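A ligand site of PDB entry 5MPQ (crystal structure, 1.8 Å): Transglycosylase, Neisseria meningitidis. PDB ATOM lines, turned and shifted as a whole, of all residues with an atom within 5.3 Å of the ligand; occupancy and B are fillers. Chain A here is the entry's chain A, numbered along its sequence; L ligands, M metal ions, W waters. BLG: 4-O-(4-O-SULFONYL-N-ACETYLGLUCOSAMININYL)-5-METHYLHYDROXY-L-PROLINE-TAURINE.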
ATOM      1  N   GLU A 441      -7.741 -27.632  11.082  1.00  0.00           N
ATOM      2  CA  GLU A 441      -7.419 -28.296   9.824  1.00  0.00           C
ATOM      3  C   GLU A 441      -7.101 -29.768  10.035  1.00  0.00           C
ATOM      4  O   GLU A 441      -7.623 -30.627   9.328  1.00  0.00           O
ATOM      5  CB  GLU A 441      -6.214 -27.623   9.141  1.00  0.00           C
ATOM      6  CG  GLU A 441      -6.476 -26.273   8.563  1.00  0.00           C
ATOM      7  CD  GLU A 441      -7.314 -26.340   7.294  1.00  0.00           C
ATOM      8  OE1 GLU A 441      -7.859 -27.434   6.962  1.00  0.00           O
ATOM      9  OE2 GLU A 441      -7.419 -25.299   6.633  1.00  0.00           O
ATOM     10  N   SER A 450      -7.163 -34.895   3.662  1.00  0.00           N
ATOM     11  CA  SER A 450      -8.598 -34.787   3.460  1.00  0.00           C
ATOM     12  C   SER A 450      -8.997 -35.546   2.198  1.00  0.00           C
ATOM     13  O   SER A 450      -8.157 -36.053   1.458  1.00  0.00           O
ATOM     14  CB  SER A 450      -9.015 -33.319   3.390  1.00  0.00           C
ATOM     15  OG  SER A 450      -8.869 -32.808   2.074  1.00  0.00           O
ATOM     16  N   ARG A 451     -10.308 -35.616   1.927  1.00  0.00           N
ATOM     17  CA  ARG A 451     -10.757 -36.372   0.756  1.00  0.00           C
ATOM     18  C   ARG A 451     -10.264 -35.730  -0.531  1.00  0.00           C
ATOM     19  O   ARG A 451      -9.920 -36.431  -1.493  1.00  0.00           O
ATOM     20  CB  ARG A 451     -12.284 -36.502   0.743  1.00  0.00           C
ATOM     21  CG  ARG A 451     -13.031 -35.243   0.384  1.00  0.00           C
ATOM     22  CD  ARG A 451     -13.481 -34.525   1.632  1.00  0.00           C
ATOM     23  NE  ARG A 451     -14.194 -33.278   1.404  1.00  0.00           N
ATOM     24  CZ  ARG A 451     -15.512 -33.183   1.225  1.00  0.00           C
ATOM     25  NH1 ARG A 451     -16.292 -34.269   1.251  1.00  0.00           N
ATOM     26  NH2 ARG A 451     -16.059 -31.988   1.035  1.00  0.00           N
ATOM     27  N   VAL A 452     -10.178 -34.385  -0.579  1.00  0.00           N
ATOM     28  CA  VAL A 452      -9.787 -33.698  -1.802  1.00  0.00           C
ATOM     29  C   VAL A 452      -8.280 -33.584  -1.939  1.00  0.00           C
ATOM     30  O   VAL A 452      -7.802 -32.991  -2.909  1.00  0.00           O
ATOM     31  CB  VAL A 452     -10.440 -32.297  -1.922  1.00  0.00           C
ATOM     32  CG1 VAL A 452     -11.948 -32.400  -1.933  1.00  0.00           C
ATOM     33  CG2 VAL A 452      -9.967 -31.361  -0.815  1.00  0.00           C
ATOM     34  N   ALA A 454      -5.972 -32.372   0.476  1.00  0.00           N
ATOM     35  CA  ALA A 454      -5.258 -31.417   1.315  1.00  0.00           C
ATOM     36  C   ALA A 454      -4.406 -32.169   2.328  1.00  0.00           C
ATOM     37  O   ALA A 454      -4.834 -33.165   2.909  1.00  0.00           O
ATOM     38  CB  ALA A 454      -6.238 -30.480   2.020  1.00  0.00           C
ATOM     39  N   MET A 458      -1.298 -28.266   8.009  1.00  0.00           N
ATOM     40  CA  MET A 458      -2.018 -27.057   7.621  1.00  0.00           C
ATOM     41  C   MET A 458      -2.926 -27.302   6.430  1.00  0.00           C
ATOM     42  O   MET A 458      -3.578 -26.373   5.954  1.00  0.00           O
ATOM     43  CB  MET A 458      -1.013 -25.939   7.373  1.00  0.00           C
ATOM     44  CG  MET A 458      -0.199 -25.641   8.636  1.00  0.00           C
ATOM     45  SD  MET A 458       0.650 -24.056   8.612  1.00  0.00           S
ATOM     46  CE  MET A 458      -0.723 -22.872   8.652  1.00  0.00           C
ATOM     47  N   GLN A 459      -3.009 -28.554   5.986  1.00  0.00           N
ATOM     48  CA  GLN A 459      -3.973 -28.999   4.984  1.00  0.00           C
ATOM     49  C   GLN A 459      -3.841 -28.148   3.726  1.00  0.00           C
ATOM     50  O   GLN A 459      -4.791 -27.521   3.238  1.00  0.00           O
ATOM     51  CB  GLN A 459      -5.387 -28.971   5.559  1.00  0.00           C
ATOM     52  CG  GLN A 459      -5.575 -30.106   6.558  1.00  0.00           C
ATOM     53  CD  GLN A 459      -5.569 -31.434   5.863  1.00  0.00           C
ATOM     54  OE1 GLN A 459      -6.575 -31.828   5.274  1.00  0.00           O
ATOM     55  NE2 GLN A 459      -4.432 -32.121   5.910  1.00  0.00           N
ATOM     56  N   VAL A 460      -2.633 -28.137   3.213  1.00  0.00           N
ATOM     57  CA  VAL A 460      -2.296 -27.399   2.003  1.00  0.00           C
ATOM     58  C   VAL A 460      -2.584 -28.287   0.805  1.00  0.00           C
ATOM     59  O   VAL A 460      -2.153 -29.437   0.759  1.00  0.00           O
ATOM     60  CB  VAL A 460      -0.833 -26.948   2.053  1.00  0.00           C
ATOM     61  CG1 VAL A 460      -0.447 -26.225   0.780  1.00  0.00           C
ATOM     62  CG2 VAL A 460      -0.606 -26.068   3.290  1.00  0.00           C
ATOM     63  N   MET A 461      -3.325 -27.767  -0.167  1.00  0.00           N
ATOM     64  CA  MET A 461      -3.587 -28.545  -1.366  1.00  0.00           C
ATOM     65  C   MET A 461      -2.299 -28.718  -2.172  1.00  0.00           C
ATOM     66  O   MET A 461      -1.452 -27.821  -2.215  1.00  0.00           O
ATOM     67  CB  MET A 461      -4.657 -27.895  -2.246  1.00  0.00           C
ATOM     68  CG  MET A 461      -6.004 -27.763  -1.564  1.00  0.00           C
ATOM     69  SD  MET A 461      -6.774 -29.361  -1.322  1.00  0.00           S
ATOM     70  CE  MET A 461      -6.833 -29.983  -3.000  1.00  0.00           C
ATOM     71  N   THR A 464      -1.947 -25.902  -4.623  1.00  0.00           N
ATOM     72  CA  THR A 464      -1.474 -24.700  -3.931  1.00  0.00           C
ATOM     73  C   THR A 464       0.002 -24.801  -3.548  1.00  0.00           C
ATOM     74  O   THR A 464       0.743 -23.811  -3.604  1.00  0.00           O
ATOM     75  CB  THR A 464      -2.331 -24.472  -2.685  1.00  0.00           C
ATOM     76  OG1 THR A 464      -3.707 -24.477  -3.072  1.00  0.00           O
ATOM     77  CG2 THR A 464      -1.955 -23.167  -1.976  1.00  0.00           C
ATOM     78  N   GLU A 467       2.081 -23.589  -6.451  1.00  0.00           N
ATOM     79  CA  GLU A 467       2.211 -22.131  -6.542  1.00  0.00           C
ATOM     80  C   GLU A 467       3.140 -21.580  -5.471  1.00  0.00           C
ATOM     81  O   GLU A 467       4.047 -20.808  -5.770  1.00  0.00           O
ATOM     82  CB  GLU A 467       0.856 -21.431  -6.463  1.00  0.00           C
ATOM     83  CG  GLU A 467      -0.041 -21.621  -7.665  1.00  0.00           C
ATOM     84  CD  GLU A 467      -1.167 -22.603  -7.430  1.00  0.00           C
ATOM     85  OE1 GLU A 467      -0.908 -23.809  -7.533  1.00  0.00           O
ATOM     86  OE2 GLU A 467      -2.312 -22.150  -7.165  1.00  0.00           O
ATOM     87  N   TYR A 492       1.137 -19.084   3.106  1.00  0.00           N
ATOM     88  CA  TYR A 492      -0.120 -18.939   2.407  1.00  0.00           C
ATOM     89  C   TYR A 492      -1.107 -18.138   3.237  1.00  0.00           C
ATOM     90  O   TYR A 492      -1.826 -17.304   2.694  1.00  0.00           O
ATOM     91  CB  TYR A 492      -0.702 -20.306   2.035  1.00  0.00           C
ATOM     92  CG  TYR A 492      -1.796 -20.220   1.001  1.00  0.00           C
ATOM     93  CD1 TYR A 492      -1.551 -19.750  -0.293  1.00  0.00           C
ATOM     94  CD2 TYR A 492      -3.096 -20.619   1.307  1.00  0.00           C
ATOM     95  CE1 TYR A 492      -2.587 -19.685  -1.242  1.00  0.00           C
ATOM     96  CE2 TYR A 492      -4.129 -20.557   0.370  1.00  0.00           C
ATOM     97  CZ  TYR A 492      -3.873 -20.082  -0.902  1.00  0.00           C
ATOM     98  OH  TYR A 492      -4.925 -20.022  -1.819  1.00  0.00           O
ATOM     99  N   GLY A 510     -10.494 -17.181   2.902  1.00  0.00           N
ATOM    100  CA  GLY A 510      -9.748 -17.399   1.668  1.00  0.00           C
ATOM    101  C   GLY A 510      -8.770 -18.551   1.740  1.00  0.00           C
ATOM    102  O   GLY A 510      -8.471 -19.172   0.713  1.00  0.00           O
ATOM    103  N   TYR A 511      -8.252 -18.860   2.938  1.00  0.00           N
ATOM    104  CA  TYR A 511      -7.407 -20.050   3.083  1.00  0.00           C
ATOM    105  C   TYR A 511      -8.174 -21.309   2.701  1.00  0.00           C
ATOM    106  O   TYR A 511      -7.647 -22.199   2.015  1.00  0.00           O
ATOM    107  CB  TYR A 511      -6.871 -20.149   4.522  1.00  0.00           C
ATOM    108  CG  TYR A 511      -5.772 -21.177   4.768  1.00  0.00           C
ATOM    109  CD1 TYR A 511      -6.086 -22.506   5.082  1.00  0.00           C
ATOM    110  CD2 TYR A 511      -4.435 -20.809   4.725  1.00  0.00           C
ATOM    111  CE1 TYR A 511      -5.069 -23.458   5.327  1.00  0.00           C
ATOM    112  CE2 TYR A 511      -3.412 -21.732   4.968  1.00  0.00           C
ATOM    113  CZ  TYR A 511      -3.726 -23.044   5.264  1.00  0.00           C
ATOM    114  OH  TYR A 511      -2.707 -23.959   5.525  1.00  0.00           O
ATOM    115  N   ASN A 512      -9.444 -21.378   3.088  1.00  0.00           N
ATOM    116  CA  ASN A 512     -10.266 -22.570   2.899  1.00  0.00           C
ATOM    117  C   ASN A 512     -10.995 -22.598   1.564  1.00  0.00           C
ATOM    118  O   ASN A 512     -11.057 -23.651   0.925  1.00  0.00           O
ATOM    119  CB  ASN A 512     -11.290 -22.685   4.039  1.00  0.00           C
ATOM    120  CG  ASN A 512     -12.234 -23.852   3.854  1.00  0.00           C
ATOM    121  OD1 ASN A 512     -13.375 -23.694   3.399  1.00  0.00           O
ATOM    122  ND2 ASN A 512     -11.764 -25.048   4.187  1.00  0.00           N
ATOM    123  N   ALA A 513     -11.537 -21.457   1.122  1.00  0.00           N
ATOM    124  CA  ALA A 513     -12.307 -21.378  -0.112  1.00  0.00           C
ATOM    125  C   ALA A 513     -11.543 -20.749  -1.274  1.00  0.00           C
ATOM    126  O   ALA A 513     -11.996 -20.864  -2.430  1.00  0.00           O
ATOM    127  CB  ALA A 513     -13.595 -20.582   0.134  1.00  0.00           C
ATOM    128  N   GLY A 514     -10.408 -20.114  -1.036  1.00  0.00           N
ATOM    129  CA  GLY A 514      -9.686 -19.411  -2.060  1.00  0.00           C
ATOM    130  C   GLY A 514      -9.970 -17.920  -1.987  1.00  0.00           C
ATOM    131  O   GLY A 514     -11.099 -17.499  -1.751  1.00  0.00           O
ATOM    132  N   PRO A 515      -8.936 -17.103  -2.164  1.00  0.00           N
ATOM    133  CA  PRO A 515      -9.138 -15.654  -2.004  1.00  0.00           C
ATOM    134  C   PRO A 515     -10.185 -15.067  -2.931  1.00  0.00           C
ATOM    135  O   PRO A 515     -10.887 -14.124  -2.538  1.00  0.00           O
ATOM    136  CB  PRO A 515      -7.742 -15.078  -2.274  1.00  0.00           C
ATOM    137  CG  PRO A 515      -7.037 -16.126  -3.083  1.00  0.00           C
ATOM    138  CD  PRO A 515      -7.572 -17.445  -2.598  1.00  0.00           C
ATOM    139  N   GLY A 516     -10.358 -15.627  -4.135  1.00  0.00           N
ATOM    140  CA  GLY A 516     -11.348 -15.074  -5.049  1.00  0.00           C
ATOM    141  C   GLY A 516     -12.761 -15.236  -4.556  1.00  0.00           C
ATOM    142  O   GLY A 516     -13.618 -14.361  -4.753  1.00  0.00           O
ATOM    143  N   ARG A 517     -13.053 -16.362  -3.897  1.00  0.00           N
ATOM    144  CA  ARG A 517     -14.374 -16.560  -3.319  1.00  0.00           C
ATOM    145  C   ARG A 517     -14.564 -15.677  -2.093  1.00  0.00           C
ATOM    146  O   ARG A 517     -15.621 -15.061  -1.931  1.00  0.00           O
ATOM    147  CB  ARG A 517     -14.584 -18.035  -2.990  1.00  0.00           C
ATOM    148  CG  ARG A 517     -14.703 -18.901  -4.239  1.00  0.00           C
ATOM    149  CD  ARG A 517     -14.928 -20.354  -3.922  1.00  0.00           C
ATOM    150  NE  ARG A 517     -15.518 -21.050  -5.075  1.00  0.00           N
ATOM    151  CZ  ARG A 517     -14.840 -21.416  -6.156  1.00  0.00           C
ATOM    152  NH1 ARG A 517     -13.541 -21.152  -6.270  1.00  0.00           N
ATOM    153  NH2 ARG A 517     -15.474 -22.031  -7.152  1.00  0.00           N
ATOM    154  N   GLU A 540     -19.104 -25.381   4.579  1.00  0.00           N
ATOM    155  CA  GLU A 540     -17.802 -25.829   5.077  1.00  0.00           C
ATOM    156  C   GLU A 540     -16.920 -24.649   5.511  1.00  0.00           C
ATOM    157  O   GLU A 540     -16.287 -24.693   6.565  1.00  0.00           O
ATOM    158  CB  GLU A 540     -17.056 -26.647   4.007  1.00  0.00           C
ATOM    159  CG  GLU A 540     -15.554 -26.832   4.375  1.00  0.00           C
ATOM    160  CD  GLU A 540     -14.668 -27.319   3.225  1.00  0.00           C
ATOM    161  OE1 GLU A 540     -15.185 -27.532   2.114  1.00  0.00           O
ATOM    162  OE2 GLU A 540     -13.449 -27.475   3.438  1.00  0.00           O
ATOM    163  N   TYR A 544     -15.861 -23.368   9.225  1.00  0.00           N
ATOM    164  CA  TYR A 544     -14.403 -23.308   9.391  1.00  0.00           C
ATOM    165  C   TYR A 544     -13.928 -21.962   9.954  1.00  0.00           C
ATOM    166  O   TYR A 544     -13.098 -21.927  10.883  1.00  0.00           O
ATOM    167  CB  TYR A 544     -13.766 -23.565   8.025  1.00  0.00           C
ATOM    168  CG  TYR A 544     -12.268 -23.427   7.942  1.00  0.00           C
ATOM    169  CD1 TYR A 544     -11.440 -24.524   8.132  1.00  0.00           C
ATOM    170  CD2 TYR A 544     -11.695 -22.213   7.629  1.00  0.00           C
ATOM    171  CE1 TYR A 544     -10.082 -24.409   8.037  1.00  0.00           C
ATOM    172  CE2 TYR A 544     -10.333 -22.085   7.529  1.00  0.00           C
ATOM    173  CZ  TYR A 544      -9.530 -23.177   7.736  1.00  0.00           C
ATOM    174  OH  TYR A 544      -8.170 -23.045   7.645  1.00  0.00           O
HETATM  175  C1  BLG L   1      -8.057 -24.714  -0.219  1.00  0.00           C
HETATM  176  C2  BLG L   1      -6.762 -24.103  -0.762  1.00  0.00           C
HETATM  177  C3  BLG L   1      -6.921 -22.922  -1.658  1.00  0.00           C
HETATM  178  C4  BLG L   1      -7.972 -23.155  -2.700  1.00  0.00           C
HETATM  179  C5  BLG L   1      -9.236 -23.807  -2.101  1.00  0.00           C
HETATM  180  O5  BLG L   1      -8.934 -25.036  -1.349  1.00  0.00           O
HETATM  181  O1  BLG L   1      -7.751 -25.893   0.423  1.00  0.00           O
HETATM  182  N2  BLG L   1      -6.035 -23.672   0.462  1.00  0.00           N
HETATM  183  C7  BLG L   1      -4.730 -24.274   0.674  1.00  0.00           C
HETATM  184  O7  BLG L   1      -4.287 -25.064  -0.112  1.00  0.00           O
HETATM  185  C8  BLG L   1      -3.983 -23.828   1.951  1.00  0.00           C
HETATM  186  O3  BLG L   1      -5.622 -22.611  -2.245  1.00  0.00           O
HETATM  187  O4  BLG L   1      -8.388 -21.887  -3.211  1.00  0.00           O
HETATM  188  S4  BLG L   1      -8.105 -21.640  -4.842  1.00  0.00           S
HETATM  189  O41 BLG L   1      -8.851 -22.656  -5.680  1.00  0.00           O
HETATM  190  O42 BLG L   1      -6.658 -21.946  -5.190  1.00  0.00           O
HETATM  191  O43 BLG L   1      -8.497 -20.232  -5.223  1.00  0.00           O
HETATM  192  C6  BLG L   1     -10.223 -24.169  -3.164  1.00  0.00           C
HETATM  193  O6  BLG L   1      -9.683 -25.168  -3.922  1.00  0.00           O
HETATM  194  CA  BLG L   1      -7.915 -26.789   2.490  1.00  0.00           C
HETATM  195  CB  BLG L   1      -8.643 -26.260   1.472  1.00  0.00           C
HETATM  196  CG  BLG L   1      -9.498 -27.568   0.989  1.00  0.00           C
HETATM  197  CD  BLG L   1     -10.044 -27.971   2.173  1.00  0.00           C
HETATM  198  N   BLG L   1      -8.882 -27.806   3.195  1.00  0.00           N
HETATM  199  C9  BLG L   1      -7.451 -25.805   3.574  1.00  0.00           C
HETATM  200  O9  BLG L   1      -8.570 -25.125   4.151  1.00  0.00           O
HETATM  201  C10 BLG L   1     -10.481 -29.432   2.251  1.00  0.00           C
HETATM  202  O10 BLG L   1      -9.690 -30.325   2.181  1.00  0.00           O
HETATM  203  N3  BLG L   1     -11.912 -29.709   2.483  1.00  0.00           N
HETATM  204  C11 BLG L   1     -12.383 -31.099   2.635  1.00  0.00           C
HETATM  205  C12 BLG L   1     -12.033 -31.437   4.161  1.00  0.00           C
HETATM  206  S   BLG L   1     -12.730 -33.040   4.691  1.00  0.00           S
HETATM  207  OS1 BLG L   1     -12.638 -33.156   6.190  1.00  0.00           O
HETATM  208  OS2 BLG L   1     -11.888 -34.209   4.220  1.00  0.00           O
HETATM  209  OS3 BLG L   1     -14.165 -33.140   4.205  1.00  0.00           O
HETATM  210 MG    MG M   1     -10.517 -30.804   8.474  1.00  0.00          MG
HETATM  211  O   HOH W   1      -5.186 -24.352  -5.285  1.00  0.00           O
HETATM  212  O   HOH W   2     -10.642 -27.466   5.797  1.00  0.00           O
HETATM  213  O   HOH W   3     -11.608 -18.957  -4.818  1.00  0.00           O
HETATM  214  O   HOH W   4      -9.486 -27.672  -2.604  1.00  0.00           O
HETATM  215  O   HOH W   5      -8.757 -30.165   5.475  1.00  0.00           O
HETATM  216  O   HOH W   6      -9.128 -17.534  -5.788  1.00  0.00           O
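The backbone carbonyl oxygen (O) of Tyr 511 sits at hydrogen-bond distance from a nitrogen (N2) of the ligand, 2.7 Å away. The side-chain hydroxyl (OH) of Tyr 492 is in hydrogen-bond range of an oxygen (O3) of the ligand (2.7 Å). The side-chain hydroxyl of Thr 464 is in hydrogen-bond range of an oxygen (O3) of the ligand. N3 of the ligand is in hydrogen-bond range of OE2 of Glu 540, 2.9 Å away. NE of Arg 451 is in salt-bridge range of OS3 of the ligand, at 2.8 Å. The side-chain carboxylate (OE1) of Glu 441 is in salt-bridge range of a nitrogen (N) of the ligand, at 3.9 Å. The backbone NH (N) of Arg 451 lies close to an oxygen (OS2) of the ligand (3.1 Å). An oxygen (O7) of the ligand sits at hydrogen-bond distance from the backbone NH (N) of Met 461. O4 of the ligand sits close to N of Gly 514. The side-chain hydroxyl (OG) of Ser 450 is in hydrogen-bond range of an oxygen (O10) of the ligand (2.6 Å). The side-chain amide nitrogen (ND2) of Asn 512 lies within hydrogen-bond range of an oxygen (O9) of the ligand (3.2 Å).
Residues that only touch the ligand: Val 452 (3.2 Å), Ala 454 (3.5 Å), Gln 459 (3.2 Å), Val 460 (3.7 Å), Ala 513 (3.8 Å) and Pro 515 (3.9 Å). Hydrophobic or aromatic side chains that line the ligand: Val 452, Ala 454, Met 461, Tyr 492, Tyr 511 and Pro 515. Of the 22 residues printed, 16 come within 4 Å of the ligand. The nearest printed residue that does not touch the ligand is Tyr 544 (4.1 Å).
The side-chain carboxylate of Glu 540 sits at hydrogen-bond distance from the side-chain amide nitrogen of Asn 512 (3.0 Å). NE2 of Gln 459 is in hydrogen-bond range of O of Ala 454 (3.2 Å). OE2 of Glu 441 lies within hydrogen-bond range of OH of Tyr 544 (2.6 Å). The backbone carbonyl oxygen (O) of Met 458 is in hydrogen-bond range of the side-chain hydroxyl (OH) of Tyr 511, 2.6 Å away. The side-chain sulfur (SD) of Met 461 sits close to the backbone NH (N) of Ala 454, 3.6 Å away. The side-chain hydroxyl of Ser 450 lies within hydrogen-bond range of the backbone NH of Ala 454 (3.3 Å). OG of Ser 450 lies close to N of Val 452, 3.4 Å away.
Water W1 lies within hydrogen-bond range of the side-chain hydroxyl of Thr 464 (2.7 Å) and an oxygen (O42) of the ligand (2.8 Å). Water W6 lies within hydrogen-bond range of the backbone NH (N) of Gly 516 (2.8 Å) and an oxygen (O43) of the ligand (2.8 Å). Water W4 lies within hydrogen-bond range of O6 of the ligand and SD of Met 461. Water W2 lies within hydrogen-bond range of OE1 of Glu 441, ND2 of Asn 512 and N of the ligand. Water W5 lies within hydrogen-bond range of OE1 of Gln 459, OE1 of Glu 441 and N of the ligand. Water W3 lies within hydrogen-bond range of the backbone carbonyl oxygen of Ala 513 (3.1 Å), the backbone NH of Arg 517 (3.1 Å), an oxygen (O43) of the ligand (3.4 Å) and the backbone carbonyl oxygen of Gly 514 (3.4 Å).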
